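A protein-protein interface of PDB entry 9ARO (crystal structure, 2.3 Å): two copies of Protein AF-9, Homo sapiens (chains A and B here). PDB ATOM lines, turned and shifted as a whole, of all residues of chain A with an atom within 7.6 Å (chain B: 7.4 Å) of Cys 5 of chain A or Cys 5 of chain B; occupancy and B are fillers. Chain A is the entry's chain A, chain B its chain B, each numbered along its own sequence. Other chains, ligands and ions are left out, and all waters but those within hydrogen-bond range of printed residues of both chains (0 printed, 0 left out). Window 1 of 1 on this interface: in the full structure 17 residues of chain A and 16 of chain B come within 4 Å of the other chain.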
ATOM      1  N   ALA A   2     -13.752  33.736  -8.658  1.00  0.00           N
ATOM      2  CA  ALA A   2     -15.114  34.014  -9.089  1.00  0.00           C
ATOM      3  C   ALA A   2     -15.749  32.728  -9.617  1.00  0.00           C
ATOM      4  O   ALA A   2     -16.864  32.359  -9.231  1.00  0.00           O
ATOM      5  CB  ALA A   2     -15.104  35.078 -10.151  1.00  0.00           C
ATOM      6  N   SER A   3     -14.987  32.078 -10.506  1.00  0.00           N
ATOM      7  CA  SER A   3     -15.250  30.764 -11.085  1.00  0.00           C
ATOM      8  C   SER A   3     -15.840  29.748 -10.102  1.00  0.00           C
ATOM      9  O   SER A   3     -15.185  29.328  -9.162  1.00  0.00           O
ATOM     10  CB  SER A   3     -13.958  30.220 -11.609  1.00  0.00           C
ATOM     11  OG  SER A   3     -13.104  29.887 -10.517  1.00  0.00           O
ATOM     12  N   SER A   4     -17.054  29.287 -10.378  1.00  0.00           N
ATOM     13  CA  SER A   4     -17.673  28.255  -9.579  1.00  0.00           C
ATOM     14  C   SER A   4     -17.824  26.998 -10.429  1.00  0.00           C
ATOM     15  O   SER A   4     -18.049  27.073 -11.634  1.00  0.00           O
ATOM     16  CB  SER A   4     -18.994  28.726  -9.115  1.00  0.00           C
ATOM     17  OG  SER A   4     -19.853  28.879 -10.236  1.00  0.00           O
ATOM     18  N   CYS A   5     -17.762  25.838  -9.779  1.00  0.00           N
ATOM     19  CA  CYS A   5     -17.881  24.577 -10.488  1.00  0.00           C
ATOM     20  C   CYS A   5     -18.971  23.706  -9.860  1.00  0.00           C
ATOM     21  O   CYS A   5     -19.022  23.605  -8.642  1.00  0.00           O
ATOM     22  CB  CYS A   5     -16.562  23.816 -10.428  1.00  0.00           C
ATOM     23  SG  CYS A   5     -16.464  22.497 -11.663  1.00  0.00           S
ATOM     24  N   ALA A   6     -19.797  23.057 -10.694  1.00  0.00           N
ATOM     25  CA  ALA A   6     -20.711  22.013 -10.240  1.00  0.00           C
ATOM     26  C   ALA A   6     -20.426  20.709 -10.979  1.00  0.00           C
ATOM     27  O   ALA A   6     -20.603  20.636 -12.200  1.00  0.00           O
ATOM     28  CB  ALA A   6     -22.155  22.406 -10.473  1.00  0.00           C
ATOM     29  N   VAL A   7     -20.054  19.654 -10.242  1.00  0.00           N
ATOM     30  CA  VAL A   7     -19.900  18.366 -10.898  1.00  0.00           C
ATOM     31  C   VAL A   7     -21.028  17.408 -10.520  1.00  0.00           C
ATOM     32  O   VAL A   7     -21.397  17.267  -9.350  1.00  0.00           O
ATOM     33  CB  VAL A   7     -18.541  17.755 -10.607  1.00  0.00           C
ATOM     34  CG1 VAL A   7     -18.475  16.320 -11.088  1.00  0.00           C
ATOM     35  CG2 VAL A   7     -17.448  18.608 -11.205  1.00  0.00           C
ATOM     36  N   GLN A   8     -21.566  16.785 -11.571  1.00  0.00           N
ATOM     37  CA  GLN A   8     -22.545  15.712 -11.488  1.00  0.00           C
ATOM     38  C   GLN A   8     -21.849  14.386 -11.829  1.00  0.00           C
ATOM     39  O   GLN A   8     -21.027  14.350 -12.734  1.00  0.00           O
ATOM     40  CB  GLN A   8     -23.703  16.058 -12.430  1.00  0.00           C
ATOM     41  CG  GLN A   8     -25.027  15.381 -12.112  1.00  0.00           C
ATOM     42  CD  GLN A   8     -26.155  15.935 -12.958  1.00  0.00           C
ATOM     43  OE1 GLN A   8     -26.269  15.652 -14.155  1.00  0.00           O
ATOM     44  NE2 GLN A   8     -27.028  16.694 -12.312  1.00  0.00           N
ATOM     45  N   VAL A   9     -22.134  13.321 -11.058  1.00  0.00           N
ATOM     46  CA  VAL A   9     -21.888  11.951 -11.501  1.00  0.00           C
ATOM     47  C   VAL A   9     -23.158  11.111 -11.395  1.00  0.00           C
ATOM     48  O   VAL A   9     -24.054  11.357 -10.601  1.00  0.00           O
ATOM     49  CB  VAL A   9     -20.715  11.283 -10.761  1.00  0.00           C
ATOM     50  CG1 VAL A   9     -19.402  11.969 -11.103  1.00  0.00           C
ATOM     51  CG2 VAL A   9     -20.921  11.239  -9.261  1.00  0.00           C
ATOM     52  N   THR A 123     -24.787  15.625  -7.296  1.00  0.00           N
ATOM     53  CA  THR A 123     -24.263  16.939  -7.610  1.00  0.00           C
ATOM     54  C   THR A 123     -23.322  17.377  -6.503  1.00  0.00           C
ATOM     55  O   THR A 123     -23.664  17.260  -5.334  1.00  0.00           O
ATOM     56  CB  THR A 123     -25.407  17.935  -7.781  1.00  0.00           C
ATOM     57  OG1 THR A 123     -26.282  17.265  -8.689  1.00  0.00           O
ATOM     58  CG2 THR A 123     -24.969  19.277  -8.326  1.00  0.00           C
ATOM     59  N   PHE A 124     -22.155  17.892  -6.903  1.00  0.00           N
ATOM     60  CA  PHE A 124     -21.189  18.483  -5.992  1.00  0.00           C
ATOM     61  C   PHE A 124     -20.914  19.946  -6.355  1.00  0.00           C
ATOM     62  O   PHE A 124     -20.612  20.280  -7.507  1.00  0.00           O
ATOM     63  CB  PHE A 124     -19.913  17.648  -6.051  1.00  0.00           C
ATOM     64  CG  PHE A 124     -20.037  16.283  -5.449  1.00  0.00           C
ATOM     65  CD1 PHE A 124     -19.940  16.104  -4.092  1.00  0.00           C
ATOM     66  CD2 PHE A 124     -20.221  15.175  -6.256  1.00  0.00           C
ATOM     67  CE1 PHE A 124     -20.046  14.830  -3.553  1.00  0.00           C
ATOM     68  CE2 PHE A 124     -20.367  13.907  -5.710  1.00  0.00           C
ATOM     69  CZ  PHE A 124     -20.281  13.737  -4.358  1.00  0.00           C
ATOM     70  N   ASN A 125     -20.996  20.829  -5.370  1.00  0.00           N
ATOM     71  CA  ASN A 125     -20.819  22.246  -5.621  1.00  0.00           C
ATOM     72  C   ASN A 125     -19.493  22.645  -5.011  1.00  0.00           C
ATOM     73  O   ASN A 125     -19.312  22.515  -3.804  1.00  0.00           O
ATOM     74  CB  ASN A 125     -21.969  23.105  -5.087  1.00  0.00           C
ATOM     75  CG  ASN A 125     -23.198  22.926  -5.957  1.00  0.00           C
ATOM     76  OD1 ASN A 125     -23.065  22.834  -7.180  1.00  0.00           O
ATOM     77  ND2 ASN A 125     -24.380  22.844  -5.364  1.00  0.00           N
ATOM     78  N   ASN A 126     -18.574  23.061  -5.885  1.00  0.00           N
ATOM     79  CA  ASN A 126     -17.292  23.634  -5.520  1.00  0.00           C
ATOM     80  C   ASN A 126     -16.530  22.646  -4.647  1.00  0.00           C
ATOM     81  O   ASN A 126     -16.177  22.979  -3.530  1.00  0.00           O
ATOM     82  CB  ASN A 126     -17.469  25.048  -4.954  1.00  0.00           C
ATOM     83  CG  ASN A 126     -17.904  25.991  -6.058  1.00  0.00           C
ATOM     84  OD1 ASN A 126     -17.097  26.417  -6.882  1.00  0.00           O
ATOM     85  ND2 ASN A 126     -19.196  26.239  -6.152  1.00  0.00           N
ATOM     86  N   PRO A 127     -16.270  21.405  -5.131  1.00  0.00           N
ATOM     87  CA  PRO A 127     -15.428  20.440  -4.410  1.00  0.00           C
ATOM     88  C   PRO A 127     -14.052  21.051  -4.391  1.00  0.00           C
ATOM     89  O   PRO A 127     -13.837  21.952  -5.186  1.00  0.00           O
ATOM     90  CB  PRO A 127     -15.423  19.196  -5.309  1.00  0.00           C
ATOM     91  CG  PRO A 127     -15.707  19.774  -6.686  1.00  0.00           C
ATOM     92  CD  PRO A 127     -16.750  20.850  -6.408  1.00  0.00           C
ATOM     93  N   ARG A 132     -12.427  17.241  -7.295  1.00  0.00           N
ATOM     94  CA  ARG A 132     -12.867  17.548  -8.628  1.00  0.00           C
ATOM     95  C   ARG A 132     -12.109  16.686  -9.657  1.00  0.00           C
ATOM     96  O   ARG A 132     -12.712  16.221 -10.618  1.00  0.00           O
ATOM     97  CB  ARG A 132     -12.685  19.046  -8.867  1.00  0.00           C
ATOM     98  CG  ARG A 132     -13.481  19.592 -10.052  1.00  0.00           C
ATOM     99  CD  ARG A 132     -13.125  21.018 -10.404  1.00  0.00           C
ATOM    100  NE  ARG A 132     -11.700  21.295 -10.524  1.00  0.00           N
ATOM    101  CZ  ARG A 132     -11.025  22.238  -9.863  1.00  0.00           C
ATOM    102  NH1 ARG A 132     -11.598  22.911  -8.879  1.00  0.00           N
ATOM    103  NH2 ARG A 132      -9.753  22.456 -10.170  1.00  0.00           N
ATOM    104  N   LEU A 136     -13.706  13.640 -12.122  1.00  0.00           N
ATOM    105  CA  LEU A 136     -13.774  13.918 -13.550  1.00  0.00           C
ATOM    106  C   LEU A 136     -12.842  13.031 -14.378  1.00  0.00           C
ATOM    107  O   LEU A 136     -13.082  12.878 -15.565  1.00  0.00           O
ATOM    108  CB  LEU A 136     -13.528  15.411 -13.778  1.00  0.00           C
ATOM    109  CG  LEU A 136     -14.793  16.260 -13.633  1.00  0.00           C
ATOM    110  CD1 LEU A 136     -14.490  17.723 -13.277  1.00  0.00           C
ATOM    111  CD2 LEU A 136     -15.613  16.155 -14.918  1.00  0.00           C
ATOM    112  N   ALA B   2     -19.397   9.228 -16.644  1.00  0.00           N
ATOM    113  CA  ALA B   2     -20.222   9.533 -15.489  1.00  0.00           C
ATOM    114  C   ALA B   2     -20.081  11.002 -15.111  1.00  0.00           C
ATOM    115  O   ALA B   2     -20.989  11.528 -14.495  1.00  0.00           O
ATOM    116  CB  ALA B   2     -19.877   8.627 -14.327  1.00  0.00           C
ATOM    117  N   SER B   3     -18.984  11.673 -15.491  1.00  0.00           N
ATOM    118  CA  SER B   3     -18.727  13.002 -14.963  1.00  0.00           C
ATOM    119  C   SER B   3     -19.030  14.050 -16.021  1.00  0.00           C
ATOM    120  O   SER B   3     -18.273  14.237 -16.966  1.00  0.00           O
ATOM    121  CB  SER B   3     -17.322  13.151 -14.440  1.00  0.00           C
ATOM    122  OG  SER B   3     -16.431  13.522 -15.483  1.00  0.00           O
ATOM    123  N   SER B   4     -20.138  14.744 -15.811  1.00  0.00           N
ATOM    124  CA  SER B   4     -20.338  16.045 -16.402  1.00  0.00           C
ATOM    125  C   SER B   4     -19.991  17.164 -15.405  1.00  0.00           C
ATOM    126  O   SER B   4     -20.074  17.060 -14.179  1.00  0.00           O
ATOM    127  CB  SER B   4     -21.720  16.162 -16.876  1.00  0.00           C
ATOM    128  OG  SER B   4     -22.574  16.293 -15.761  1.00  0.00           O
ATOM    129  N   CYS B   5     -19.627  18.287 -15.983  1.00  0.00           N
ATOM    130  CA  CYS B   5     -19.067  19.393 -15.257  1.00  0.00           C
ATOM    131  C   CYS B   5     -19.600  20.655 -15.917  1.00  0.00           C
ATOM    132  O   CYS B   5     -19.729  20.688 -17.137  1.00  0.00           O
ATOM    133  CB  CYS B   5     -17.555  19.354 -15.382  1.00  0.00           C
ATOM    134  SG  CYS B   5     -16.789  20.904 -14.886  1.00  0.00           S
ATOM    135  N   ALA B   6     -19.945  21.651 -15.108  1.00  0.00           N
ATOM    136  CA  ALA B   6     -20.287  22.975 -15.588  1.00  0.00           C
ATOM    137  C   ALA B   6     -19.508  24.011 -14.785  1.00  0.00           C
ATOM    138  O   ALA B   6     -19.290  23.838 -13.586  1.00  0.00           O
ATOM    139  CB  ALA B   6     -21.771  23.214 -15.453  1.00  0.00           C
ATOM    140  N   VAL B   7     -19.101  25.090 -15.451  1.00  0.00           N
ATOM    141  CA  VAL B   7     -18.407  26.165 -14.767  1.00  0.00           C
ATOM    142  C   VAL B   7     -19.010  27.499 -15.205  1.00  0.00           C
ATOM    143  O   VAL B   7     -19.126  27.784 -16.403  1.00  0.00           O
ATOM    144  CB  VAL B   7     -16.904  26.093 -15.041  1.00  0.00           C
ATOM    145  CG1 VAL B   7     -16.233  27.418 -14.754  1.00  0.00           C
ATOM    146  CG2 VAL B   7     -16.229  24.964 -14.275  1.00  0.00           C
ATOM    147  N   GLN B   8     -19.489  28.239 -14.195  1.00  0.00           N
ATOM    148  CA  GLN B   8     -19.772  29.656 -14.264  1.00  0.00           C
ATOM    149  C   GLN B   8     -18.509  30.421 -13.899  1.00  0.00           C
ATOM    150  O   GLN B   8     -17.871  30.074 -12.918  1.00  0.00           O
ATOM    151  CB  GLN B   8     -20.802  30.092 -13.208  1.00  0.00           C
ATOM    152  CG  GLN B   8     -22.232  29.644 -13.482  1.00  0.00           C
ATOM    153  CD  GLN B   8     -23.253  30.371 -12.630  1.00  0.00           C
ATOM    154  OE1 GLN B   8     -23.647  31.494 -12.917  1.00  0.00           O
ATOM    155  NE2 GLN B   8     -23.775  29.696 -11.620  1.00  0.00           N
ATOM    156  N   PHE B 124     -19.982  27.358 -18.888  1.00  0.00           N
ATOM    157  CA  PHE B 124     -19.293  26.462 -19.806  1.00  0.00           C
ATOM    158  C   PHE B 124     -19.575  24.992 -19.419  1.00  0.00           C
ATOM    159  O   PHE B 124     -19.143  24.481 -18.382  1.00  0.00           O
ATOM    160  CB  PHE B 124     -17.791  26.783 -19.828  1.00  0.00           C
ATOM    161  CG  PHE B 124     -17.390  28.169 -20.282  1.00  0.00           C
ATOM    162  CD1 PHE B 124     -17.471  29.263 -19.428  1.00  0.00           C
ATOM    163  CD2 PHE B 124     -16.899  28.379 -21.560  1.00  0.00           C
ATOM    164  CE1 PHE B 124     -17.086  30.530 -19.848  1.00  0.00           C
ATOM    165  CE2 PHE B 124     -16.512  29.643 -21.982  1.00  0.00           C
ATOM    166  CZ  PHE B 124     -16.597  30.714 -21.122  1.00  0.00           C
ATOM    167  N   ASN B 125     -20.333  24.296 -20.268  1.00  0.00           N
ATOM    168  CA  ASN B 125     -20.711  22.911 -20.013  1.00  0.00           C
ATOM    169  C   ASN B 125     -19.631  22.020 -20.626  1.00  0.00           C
ATOM    170  O   ASN B 125     -19.331  22.181 -21.809  1.00  0.00           O
ATOM    171  CB  ASN B 125     -22.100  22.572 -20.586  1.00  0.00           C
ATOM    172  CG  ASN B 125     -23.273  22.979 -19.711  1.00  0.00           C
ATOM    173  OD1 ASN B 125     -23.502  22.361 -18.674  1.00  0.00           O
ATOM    174  ND2 ASN B 125     -24.061  23.960 -20.135  1.00  0.00           N
ATOM    175  N   ASN B 126     -19.018  21.148 -19.798  1.00  0.00           N
ATOM    176  CA  ASN B 126     -18.069  20.132 -20.227  1.00  0.00           C
ATOM    177  C   ASN B 126     -17.034  20.741 -21.162  1.00  0.00           C
ATOM    178  O   ASN B 126     -16.886  20.333 -22.314  1.00  0.00           O
ATOM    179  CB  ASN B 126     -18.777  18.904 -20.817  1.00  0.00           C
ATOM    180  CG  ASN B 126     -19.474  18.146 -19.709  1.00  0.00           C
ATOM    181  OD1 ASN B 126     -18.827  17.451 -18.922  1.00  0.00           O
ATOM    182  ND2 ASN B 126     -20.768  18.381 -19.570  1.00  0.00           N
ATOM    183  N   PRO B 127     -16.230  21.698 -20.659  1.00  0.00           N
ATOM    184  CA  PRO B 127     -15.047  22.152 -21.387  1.00  0.00           C
ATOM    185  C   PRO B 127     -13.999  21.053 -21.482  1.00  0.00           C
ATOM    186  O   PRO B 127     -14.094  20.060 -20.785  1.00  0.00           O
ATOM    187  CB  PRO B 127     -14.511  23.274 -20.505  1.00  0.00           C
ATOM    188  CG  PRO B 127     -15.016  22.894 -19.122  1.00  0.00           C
ATOM    189  CD  PRO B 127     -16.406  22.354 -19.366  1.00  0.00           C
ATOM    190  N   ARG B 132     -10.877  24.089 -18.566  1.00  0.00           N
ATOM    191  CA  ARG B 132     -11.482  24.018 -17.220  1.00  0.00           C
ATOM    192  C   ARG B 132     -10.404  24.365 -16.197  1.00  0.00           C
ATOM    193  O   ARG B 132     -10.713  25.036 -15.223  1.00  0.00           O
ATOM    194  CB  ARG B 132     -12.042  22.610 -17.011  1.00  0.00           C
ATOM    195  CG  ARG B 132     -12.981  22.478 -15.821  1.00  0.00           C
ATOM    196  CD  ARG B 132     -12.786  21.183 -15.057  1.00  0.00           C
ATOM    197  NE  ARG B 132     -11.631  20.418 -15.494  1.00  0.00           N
ATOM    198  CZ  ARG B 132     -11.685  19.169 -15.936  1.00  0.00           C
ATOM    199  NH1 ARG B 132     -12.631  18.810 -16.784  1.00  0.00           N
ATOM    200  NH2 ARG B 132     -10.792  18.284 -15.535  1.00  0.00           N
ATOM    201  N   LEU B 135     -10.003  27.934 -16.397  1.00  0.00           N
ATOM    202  CA  LEU B 135     -11.199  28.560 -15.913  1.00  0.00           C
ATOM    203  C   LEU B 135     -11.145  28.592 -14.392  1.00  0.00           C
ATOM    204  O   LEU B 135     -11.690  29.490 -13.787  1.00  0.00           O
ATOM    205  CB  LEU B 135     -12.422  27.744 -16.310  1.00  0.00           C
ATOM    206  CG  LEU B 135     -12.991  27.880 -17.721  1.00  0.00           C
ATOM    207  CD1 LEU B 135     -14.186  26.948 -17.805  1.00  0.00           C
ATOM    208  CD2 LEU B 135     -13.410  29.310 -18.105  1.00  0.00           C
ATOM    209  N   LEU B 136     -10.541  27.580 -13.766  1.00  0.00           N
ATOM    210  CA  LEU B 136     -10.689  27.420 -12.328  1.00  0.00           C
ATOM    211  C   LEU B 136      -9.449  27.870 -11.532  1.00  0.00           C
ATOM    212  O   LEU B 136      -9.492  27.868 -10.298  1.00  0.00           O
ATOM    213  CB  LEU B 136     -11.067  25.959 -12.066  1.00  0.00           C
ATOM    214  CG  LEU B 136     -12.524  25.613 -12.361  1.00  0.00           C
ATOM    215  CD1 LEU B 136     -12.836  24.189 -11.946  1.00  0.00           C
ATOM    216  CD2 LEU B 136     -13.455  26.572 -11.644  1.00  0.00           C
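SG of Cys 5 of chain B is in hydrogen-bond range of SG of Cys 5 of chain A.
The backbone carbonyl oxygen (O) of Ser 4 of chain B lies within hydrogen-bond range of the backbone NH (N) of Gln 8 of chain A (3.0 Å).
The backbone NH of Ala 6 of chain A sits at hydrogen-bond distance from the backbone carbonyl oxygen of Ala 6 of chain B, at 3.0 Å.
SG of Cys 5 of chain A sits close to O of Ala 6 of chain B (3.7 Å).
The backbone carbonyl oxygen (O) of Ala 2 of chain B lies close to the backbone carbonyl oxygen (O) of Gln 8 of chain A, 3.3 Å away.
The backbone NH of Ser 4 of chain A lies within hydrogen-bond range of the backbone carbonyl oxygen of Gln 8 of chain B, at 2.8 Å.
The backbone carbonyl oxygen (O) of Leu 136 of chain A sits close to the side-chain hydroxyl (OG) of Ser 3 of chain B, at 3.4 Å.
Ser 3 of chain A touches Leu 136 of chain B, and with the chains exchanged Leu 136 of chain A touches Ser 3 of chain B.
Ser 4 of chain A touches Gln 8 of chain B, and with the chains exchanged Gln 8 of chain A touches Ser 4 of chain B.
Cys 5 of chain B touches its own counterpart, Cys 5 of chain A.
Cys 5 of chain A touches Val 7 of chain B, but with the chains exchanged Val 7 of chain A does not touch Cys 5 of chain B (4.2 Å).
Hydrophobic or aromatic side chains of chain A that line the printed part of chain B: Val 7, Val 9 and Leu 136.
Along chain A the printed residues that touch a printed residue of chain B span positions 3 to 136.
Hydrophobic or aromatic side chains of chain B that line the printed part of chain A: Val 7 and Leu 136.
CA of Ser 3 of chain A touches O of Gln 8 of chain B (3.3 Å).
Ser 3 of chain A touches Leu 135 of chain B.
OG of Ser 3 of chain A touches CD2 of Leu 136 of chain B, at 3.5 Å.
Ala 6 of chain B touches Ser 4 of chain A.
Val 7 of chain B touches Ser 4 of chain A (CA to O, 3.3 Å).
Cys 5 of chain A touches Val 7 of chain B.
Val 7 of chain A touches Ser 4 of chain B.
Ser 3 of chain B touches Gln 8 of chain A (CA to O, 3.5 Å).
CA of Val 9 of chain A touches O of Ala 2 of chain B, at 3.2 Å.
Arg 132 of chain A touches Leu 136 of chain B.
The backbone carbonyl oxygen (O) of Val 7 of chain A lies within hydrogen-bond range of the backbone NH (N) of Phe 124 of chain A, 2.6 Å away.
O of Cys 5 of chain A lies within hydrogen-bond range of N of Asn 126 of chain A (2.8 Å).
The backbone carbonyl oxygen of Cys 5 of chain B sits at hydrogen-bond distance from the backbone NH of Asn 126 of chain B (2.8 Å).
N of Phe 124 of chain B is in hydrogen-bond range of O of Val 7 of chain B, 2.7 Å away.
Of the printed residues of chain B, Cys 5 of chain A touches Cys 5, Ala 6 and Val 7.
Printed residues of chain B within 4 Å of Val 9 of chain A: Ala 2.
Phe 124 of chain A touches none of the printed residues of chain B.
Pro 127 of chain A touches none of the printed residues of chain B.
Of the printed residues of chain A, Cys 5 of chain B touches Cys 5, Ala 6 and Leu 136.
Ala 6 of chain B touches just these residues of chain A: Ser 4 (3.98 Å), Cys 5 (3.5 Å) and Ala 6 (3.0 Å).
Of the printed residues of chain A, Val 7 of chain B touches Ser 4 (3.3 Å) and Cys 5 (3.6 Å).
Of the printed residues of chain A, Leu 136 of chain B touches Ser 3 (3.5 Å) and Arg 132 (3.4 Å).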
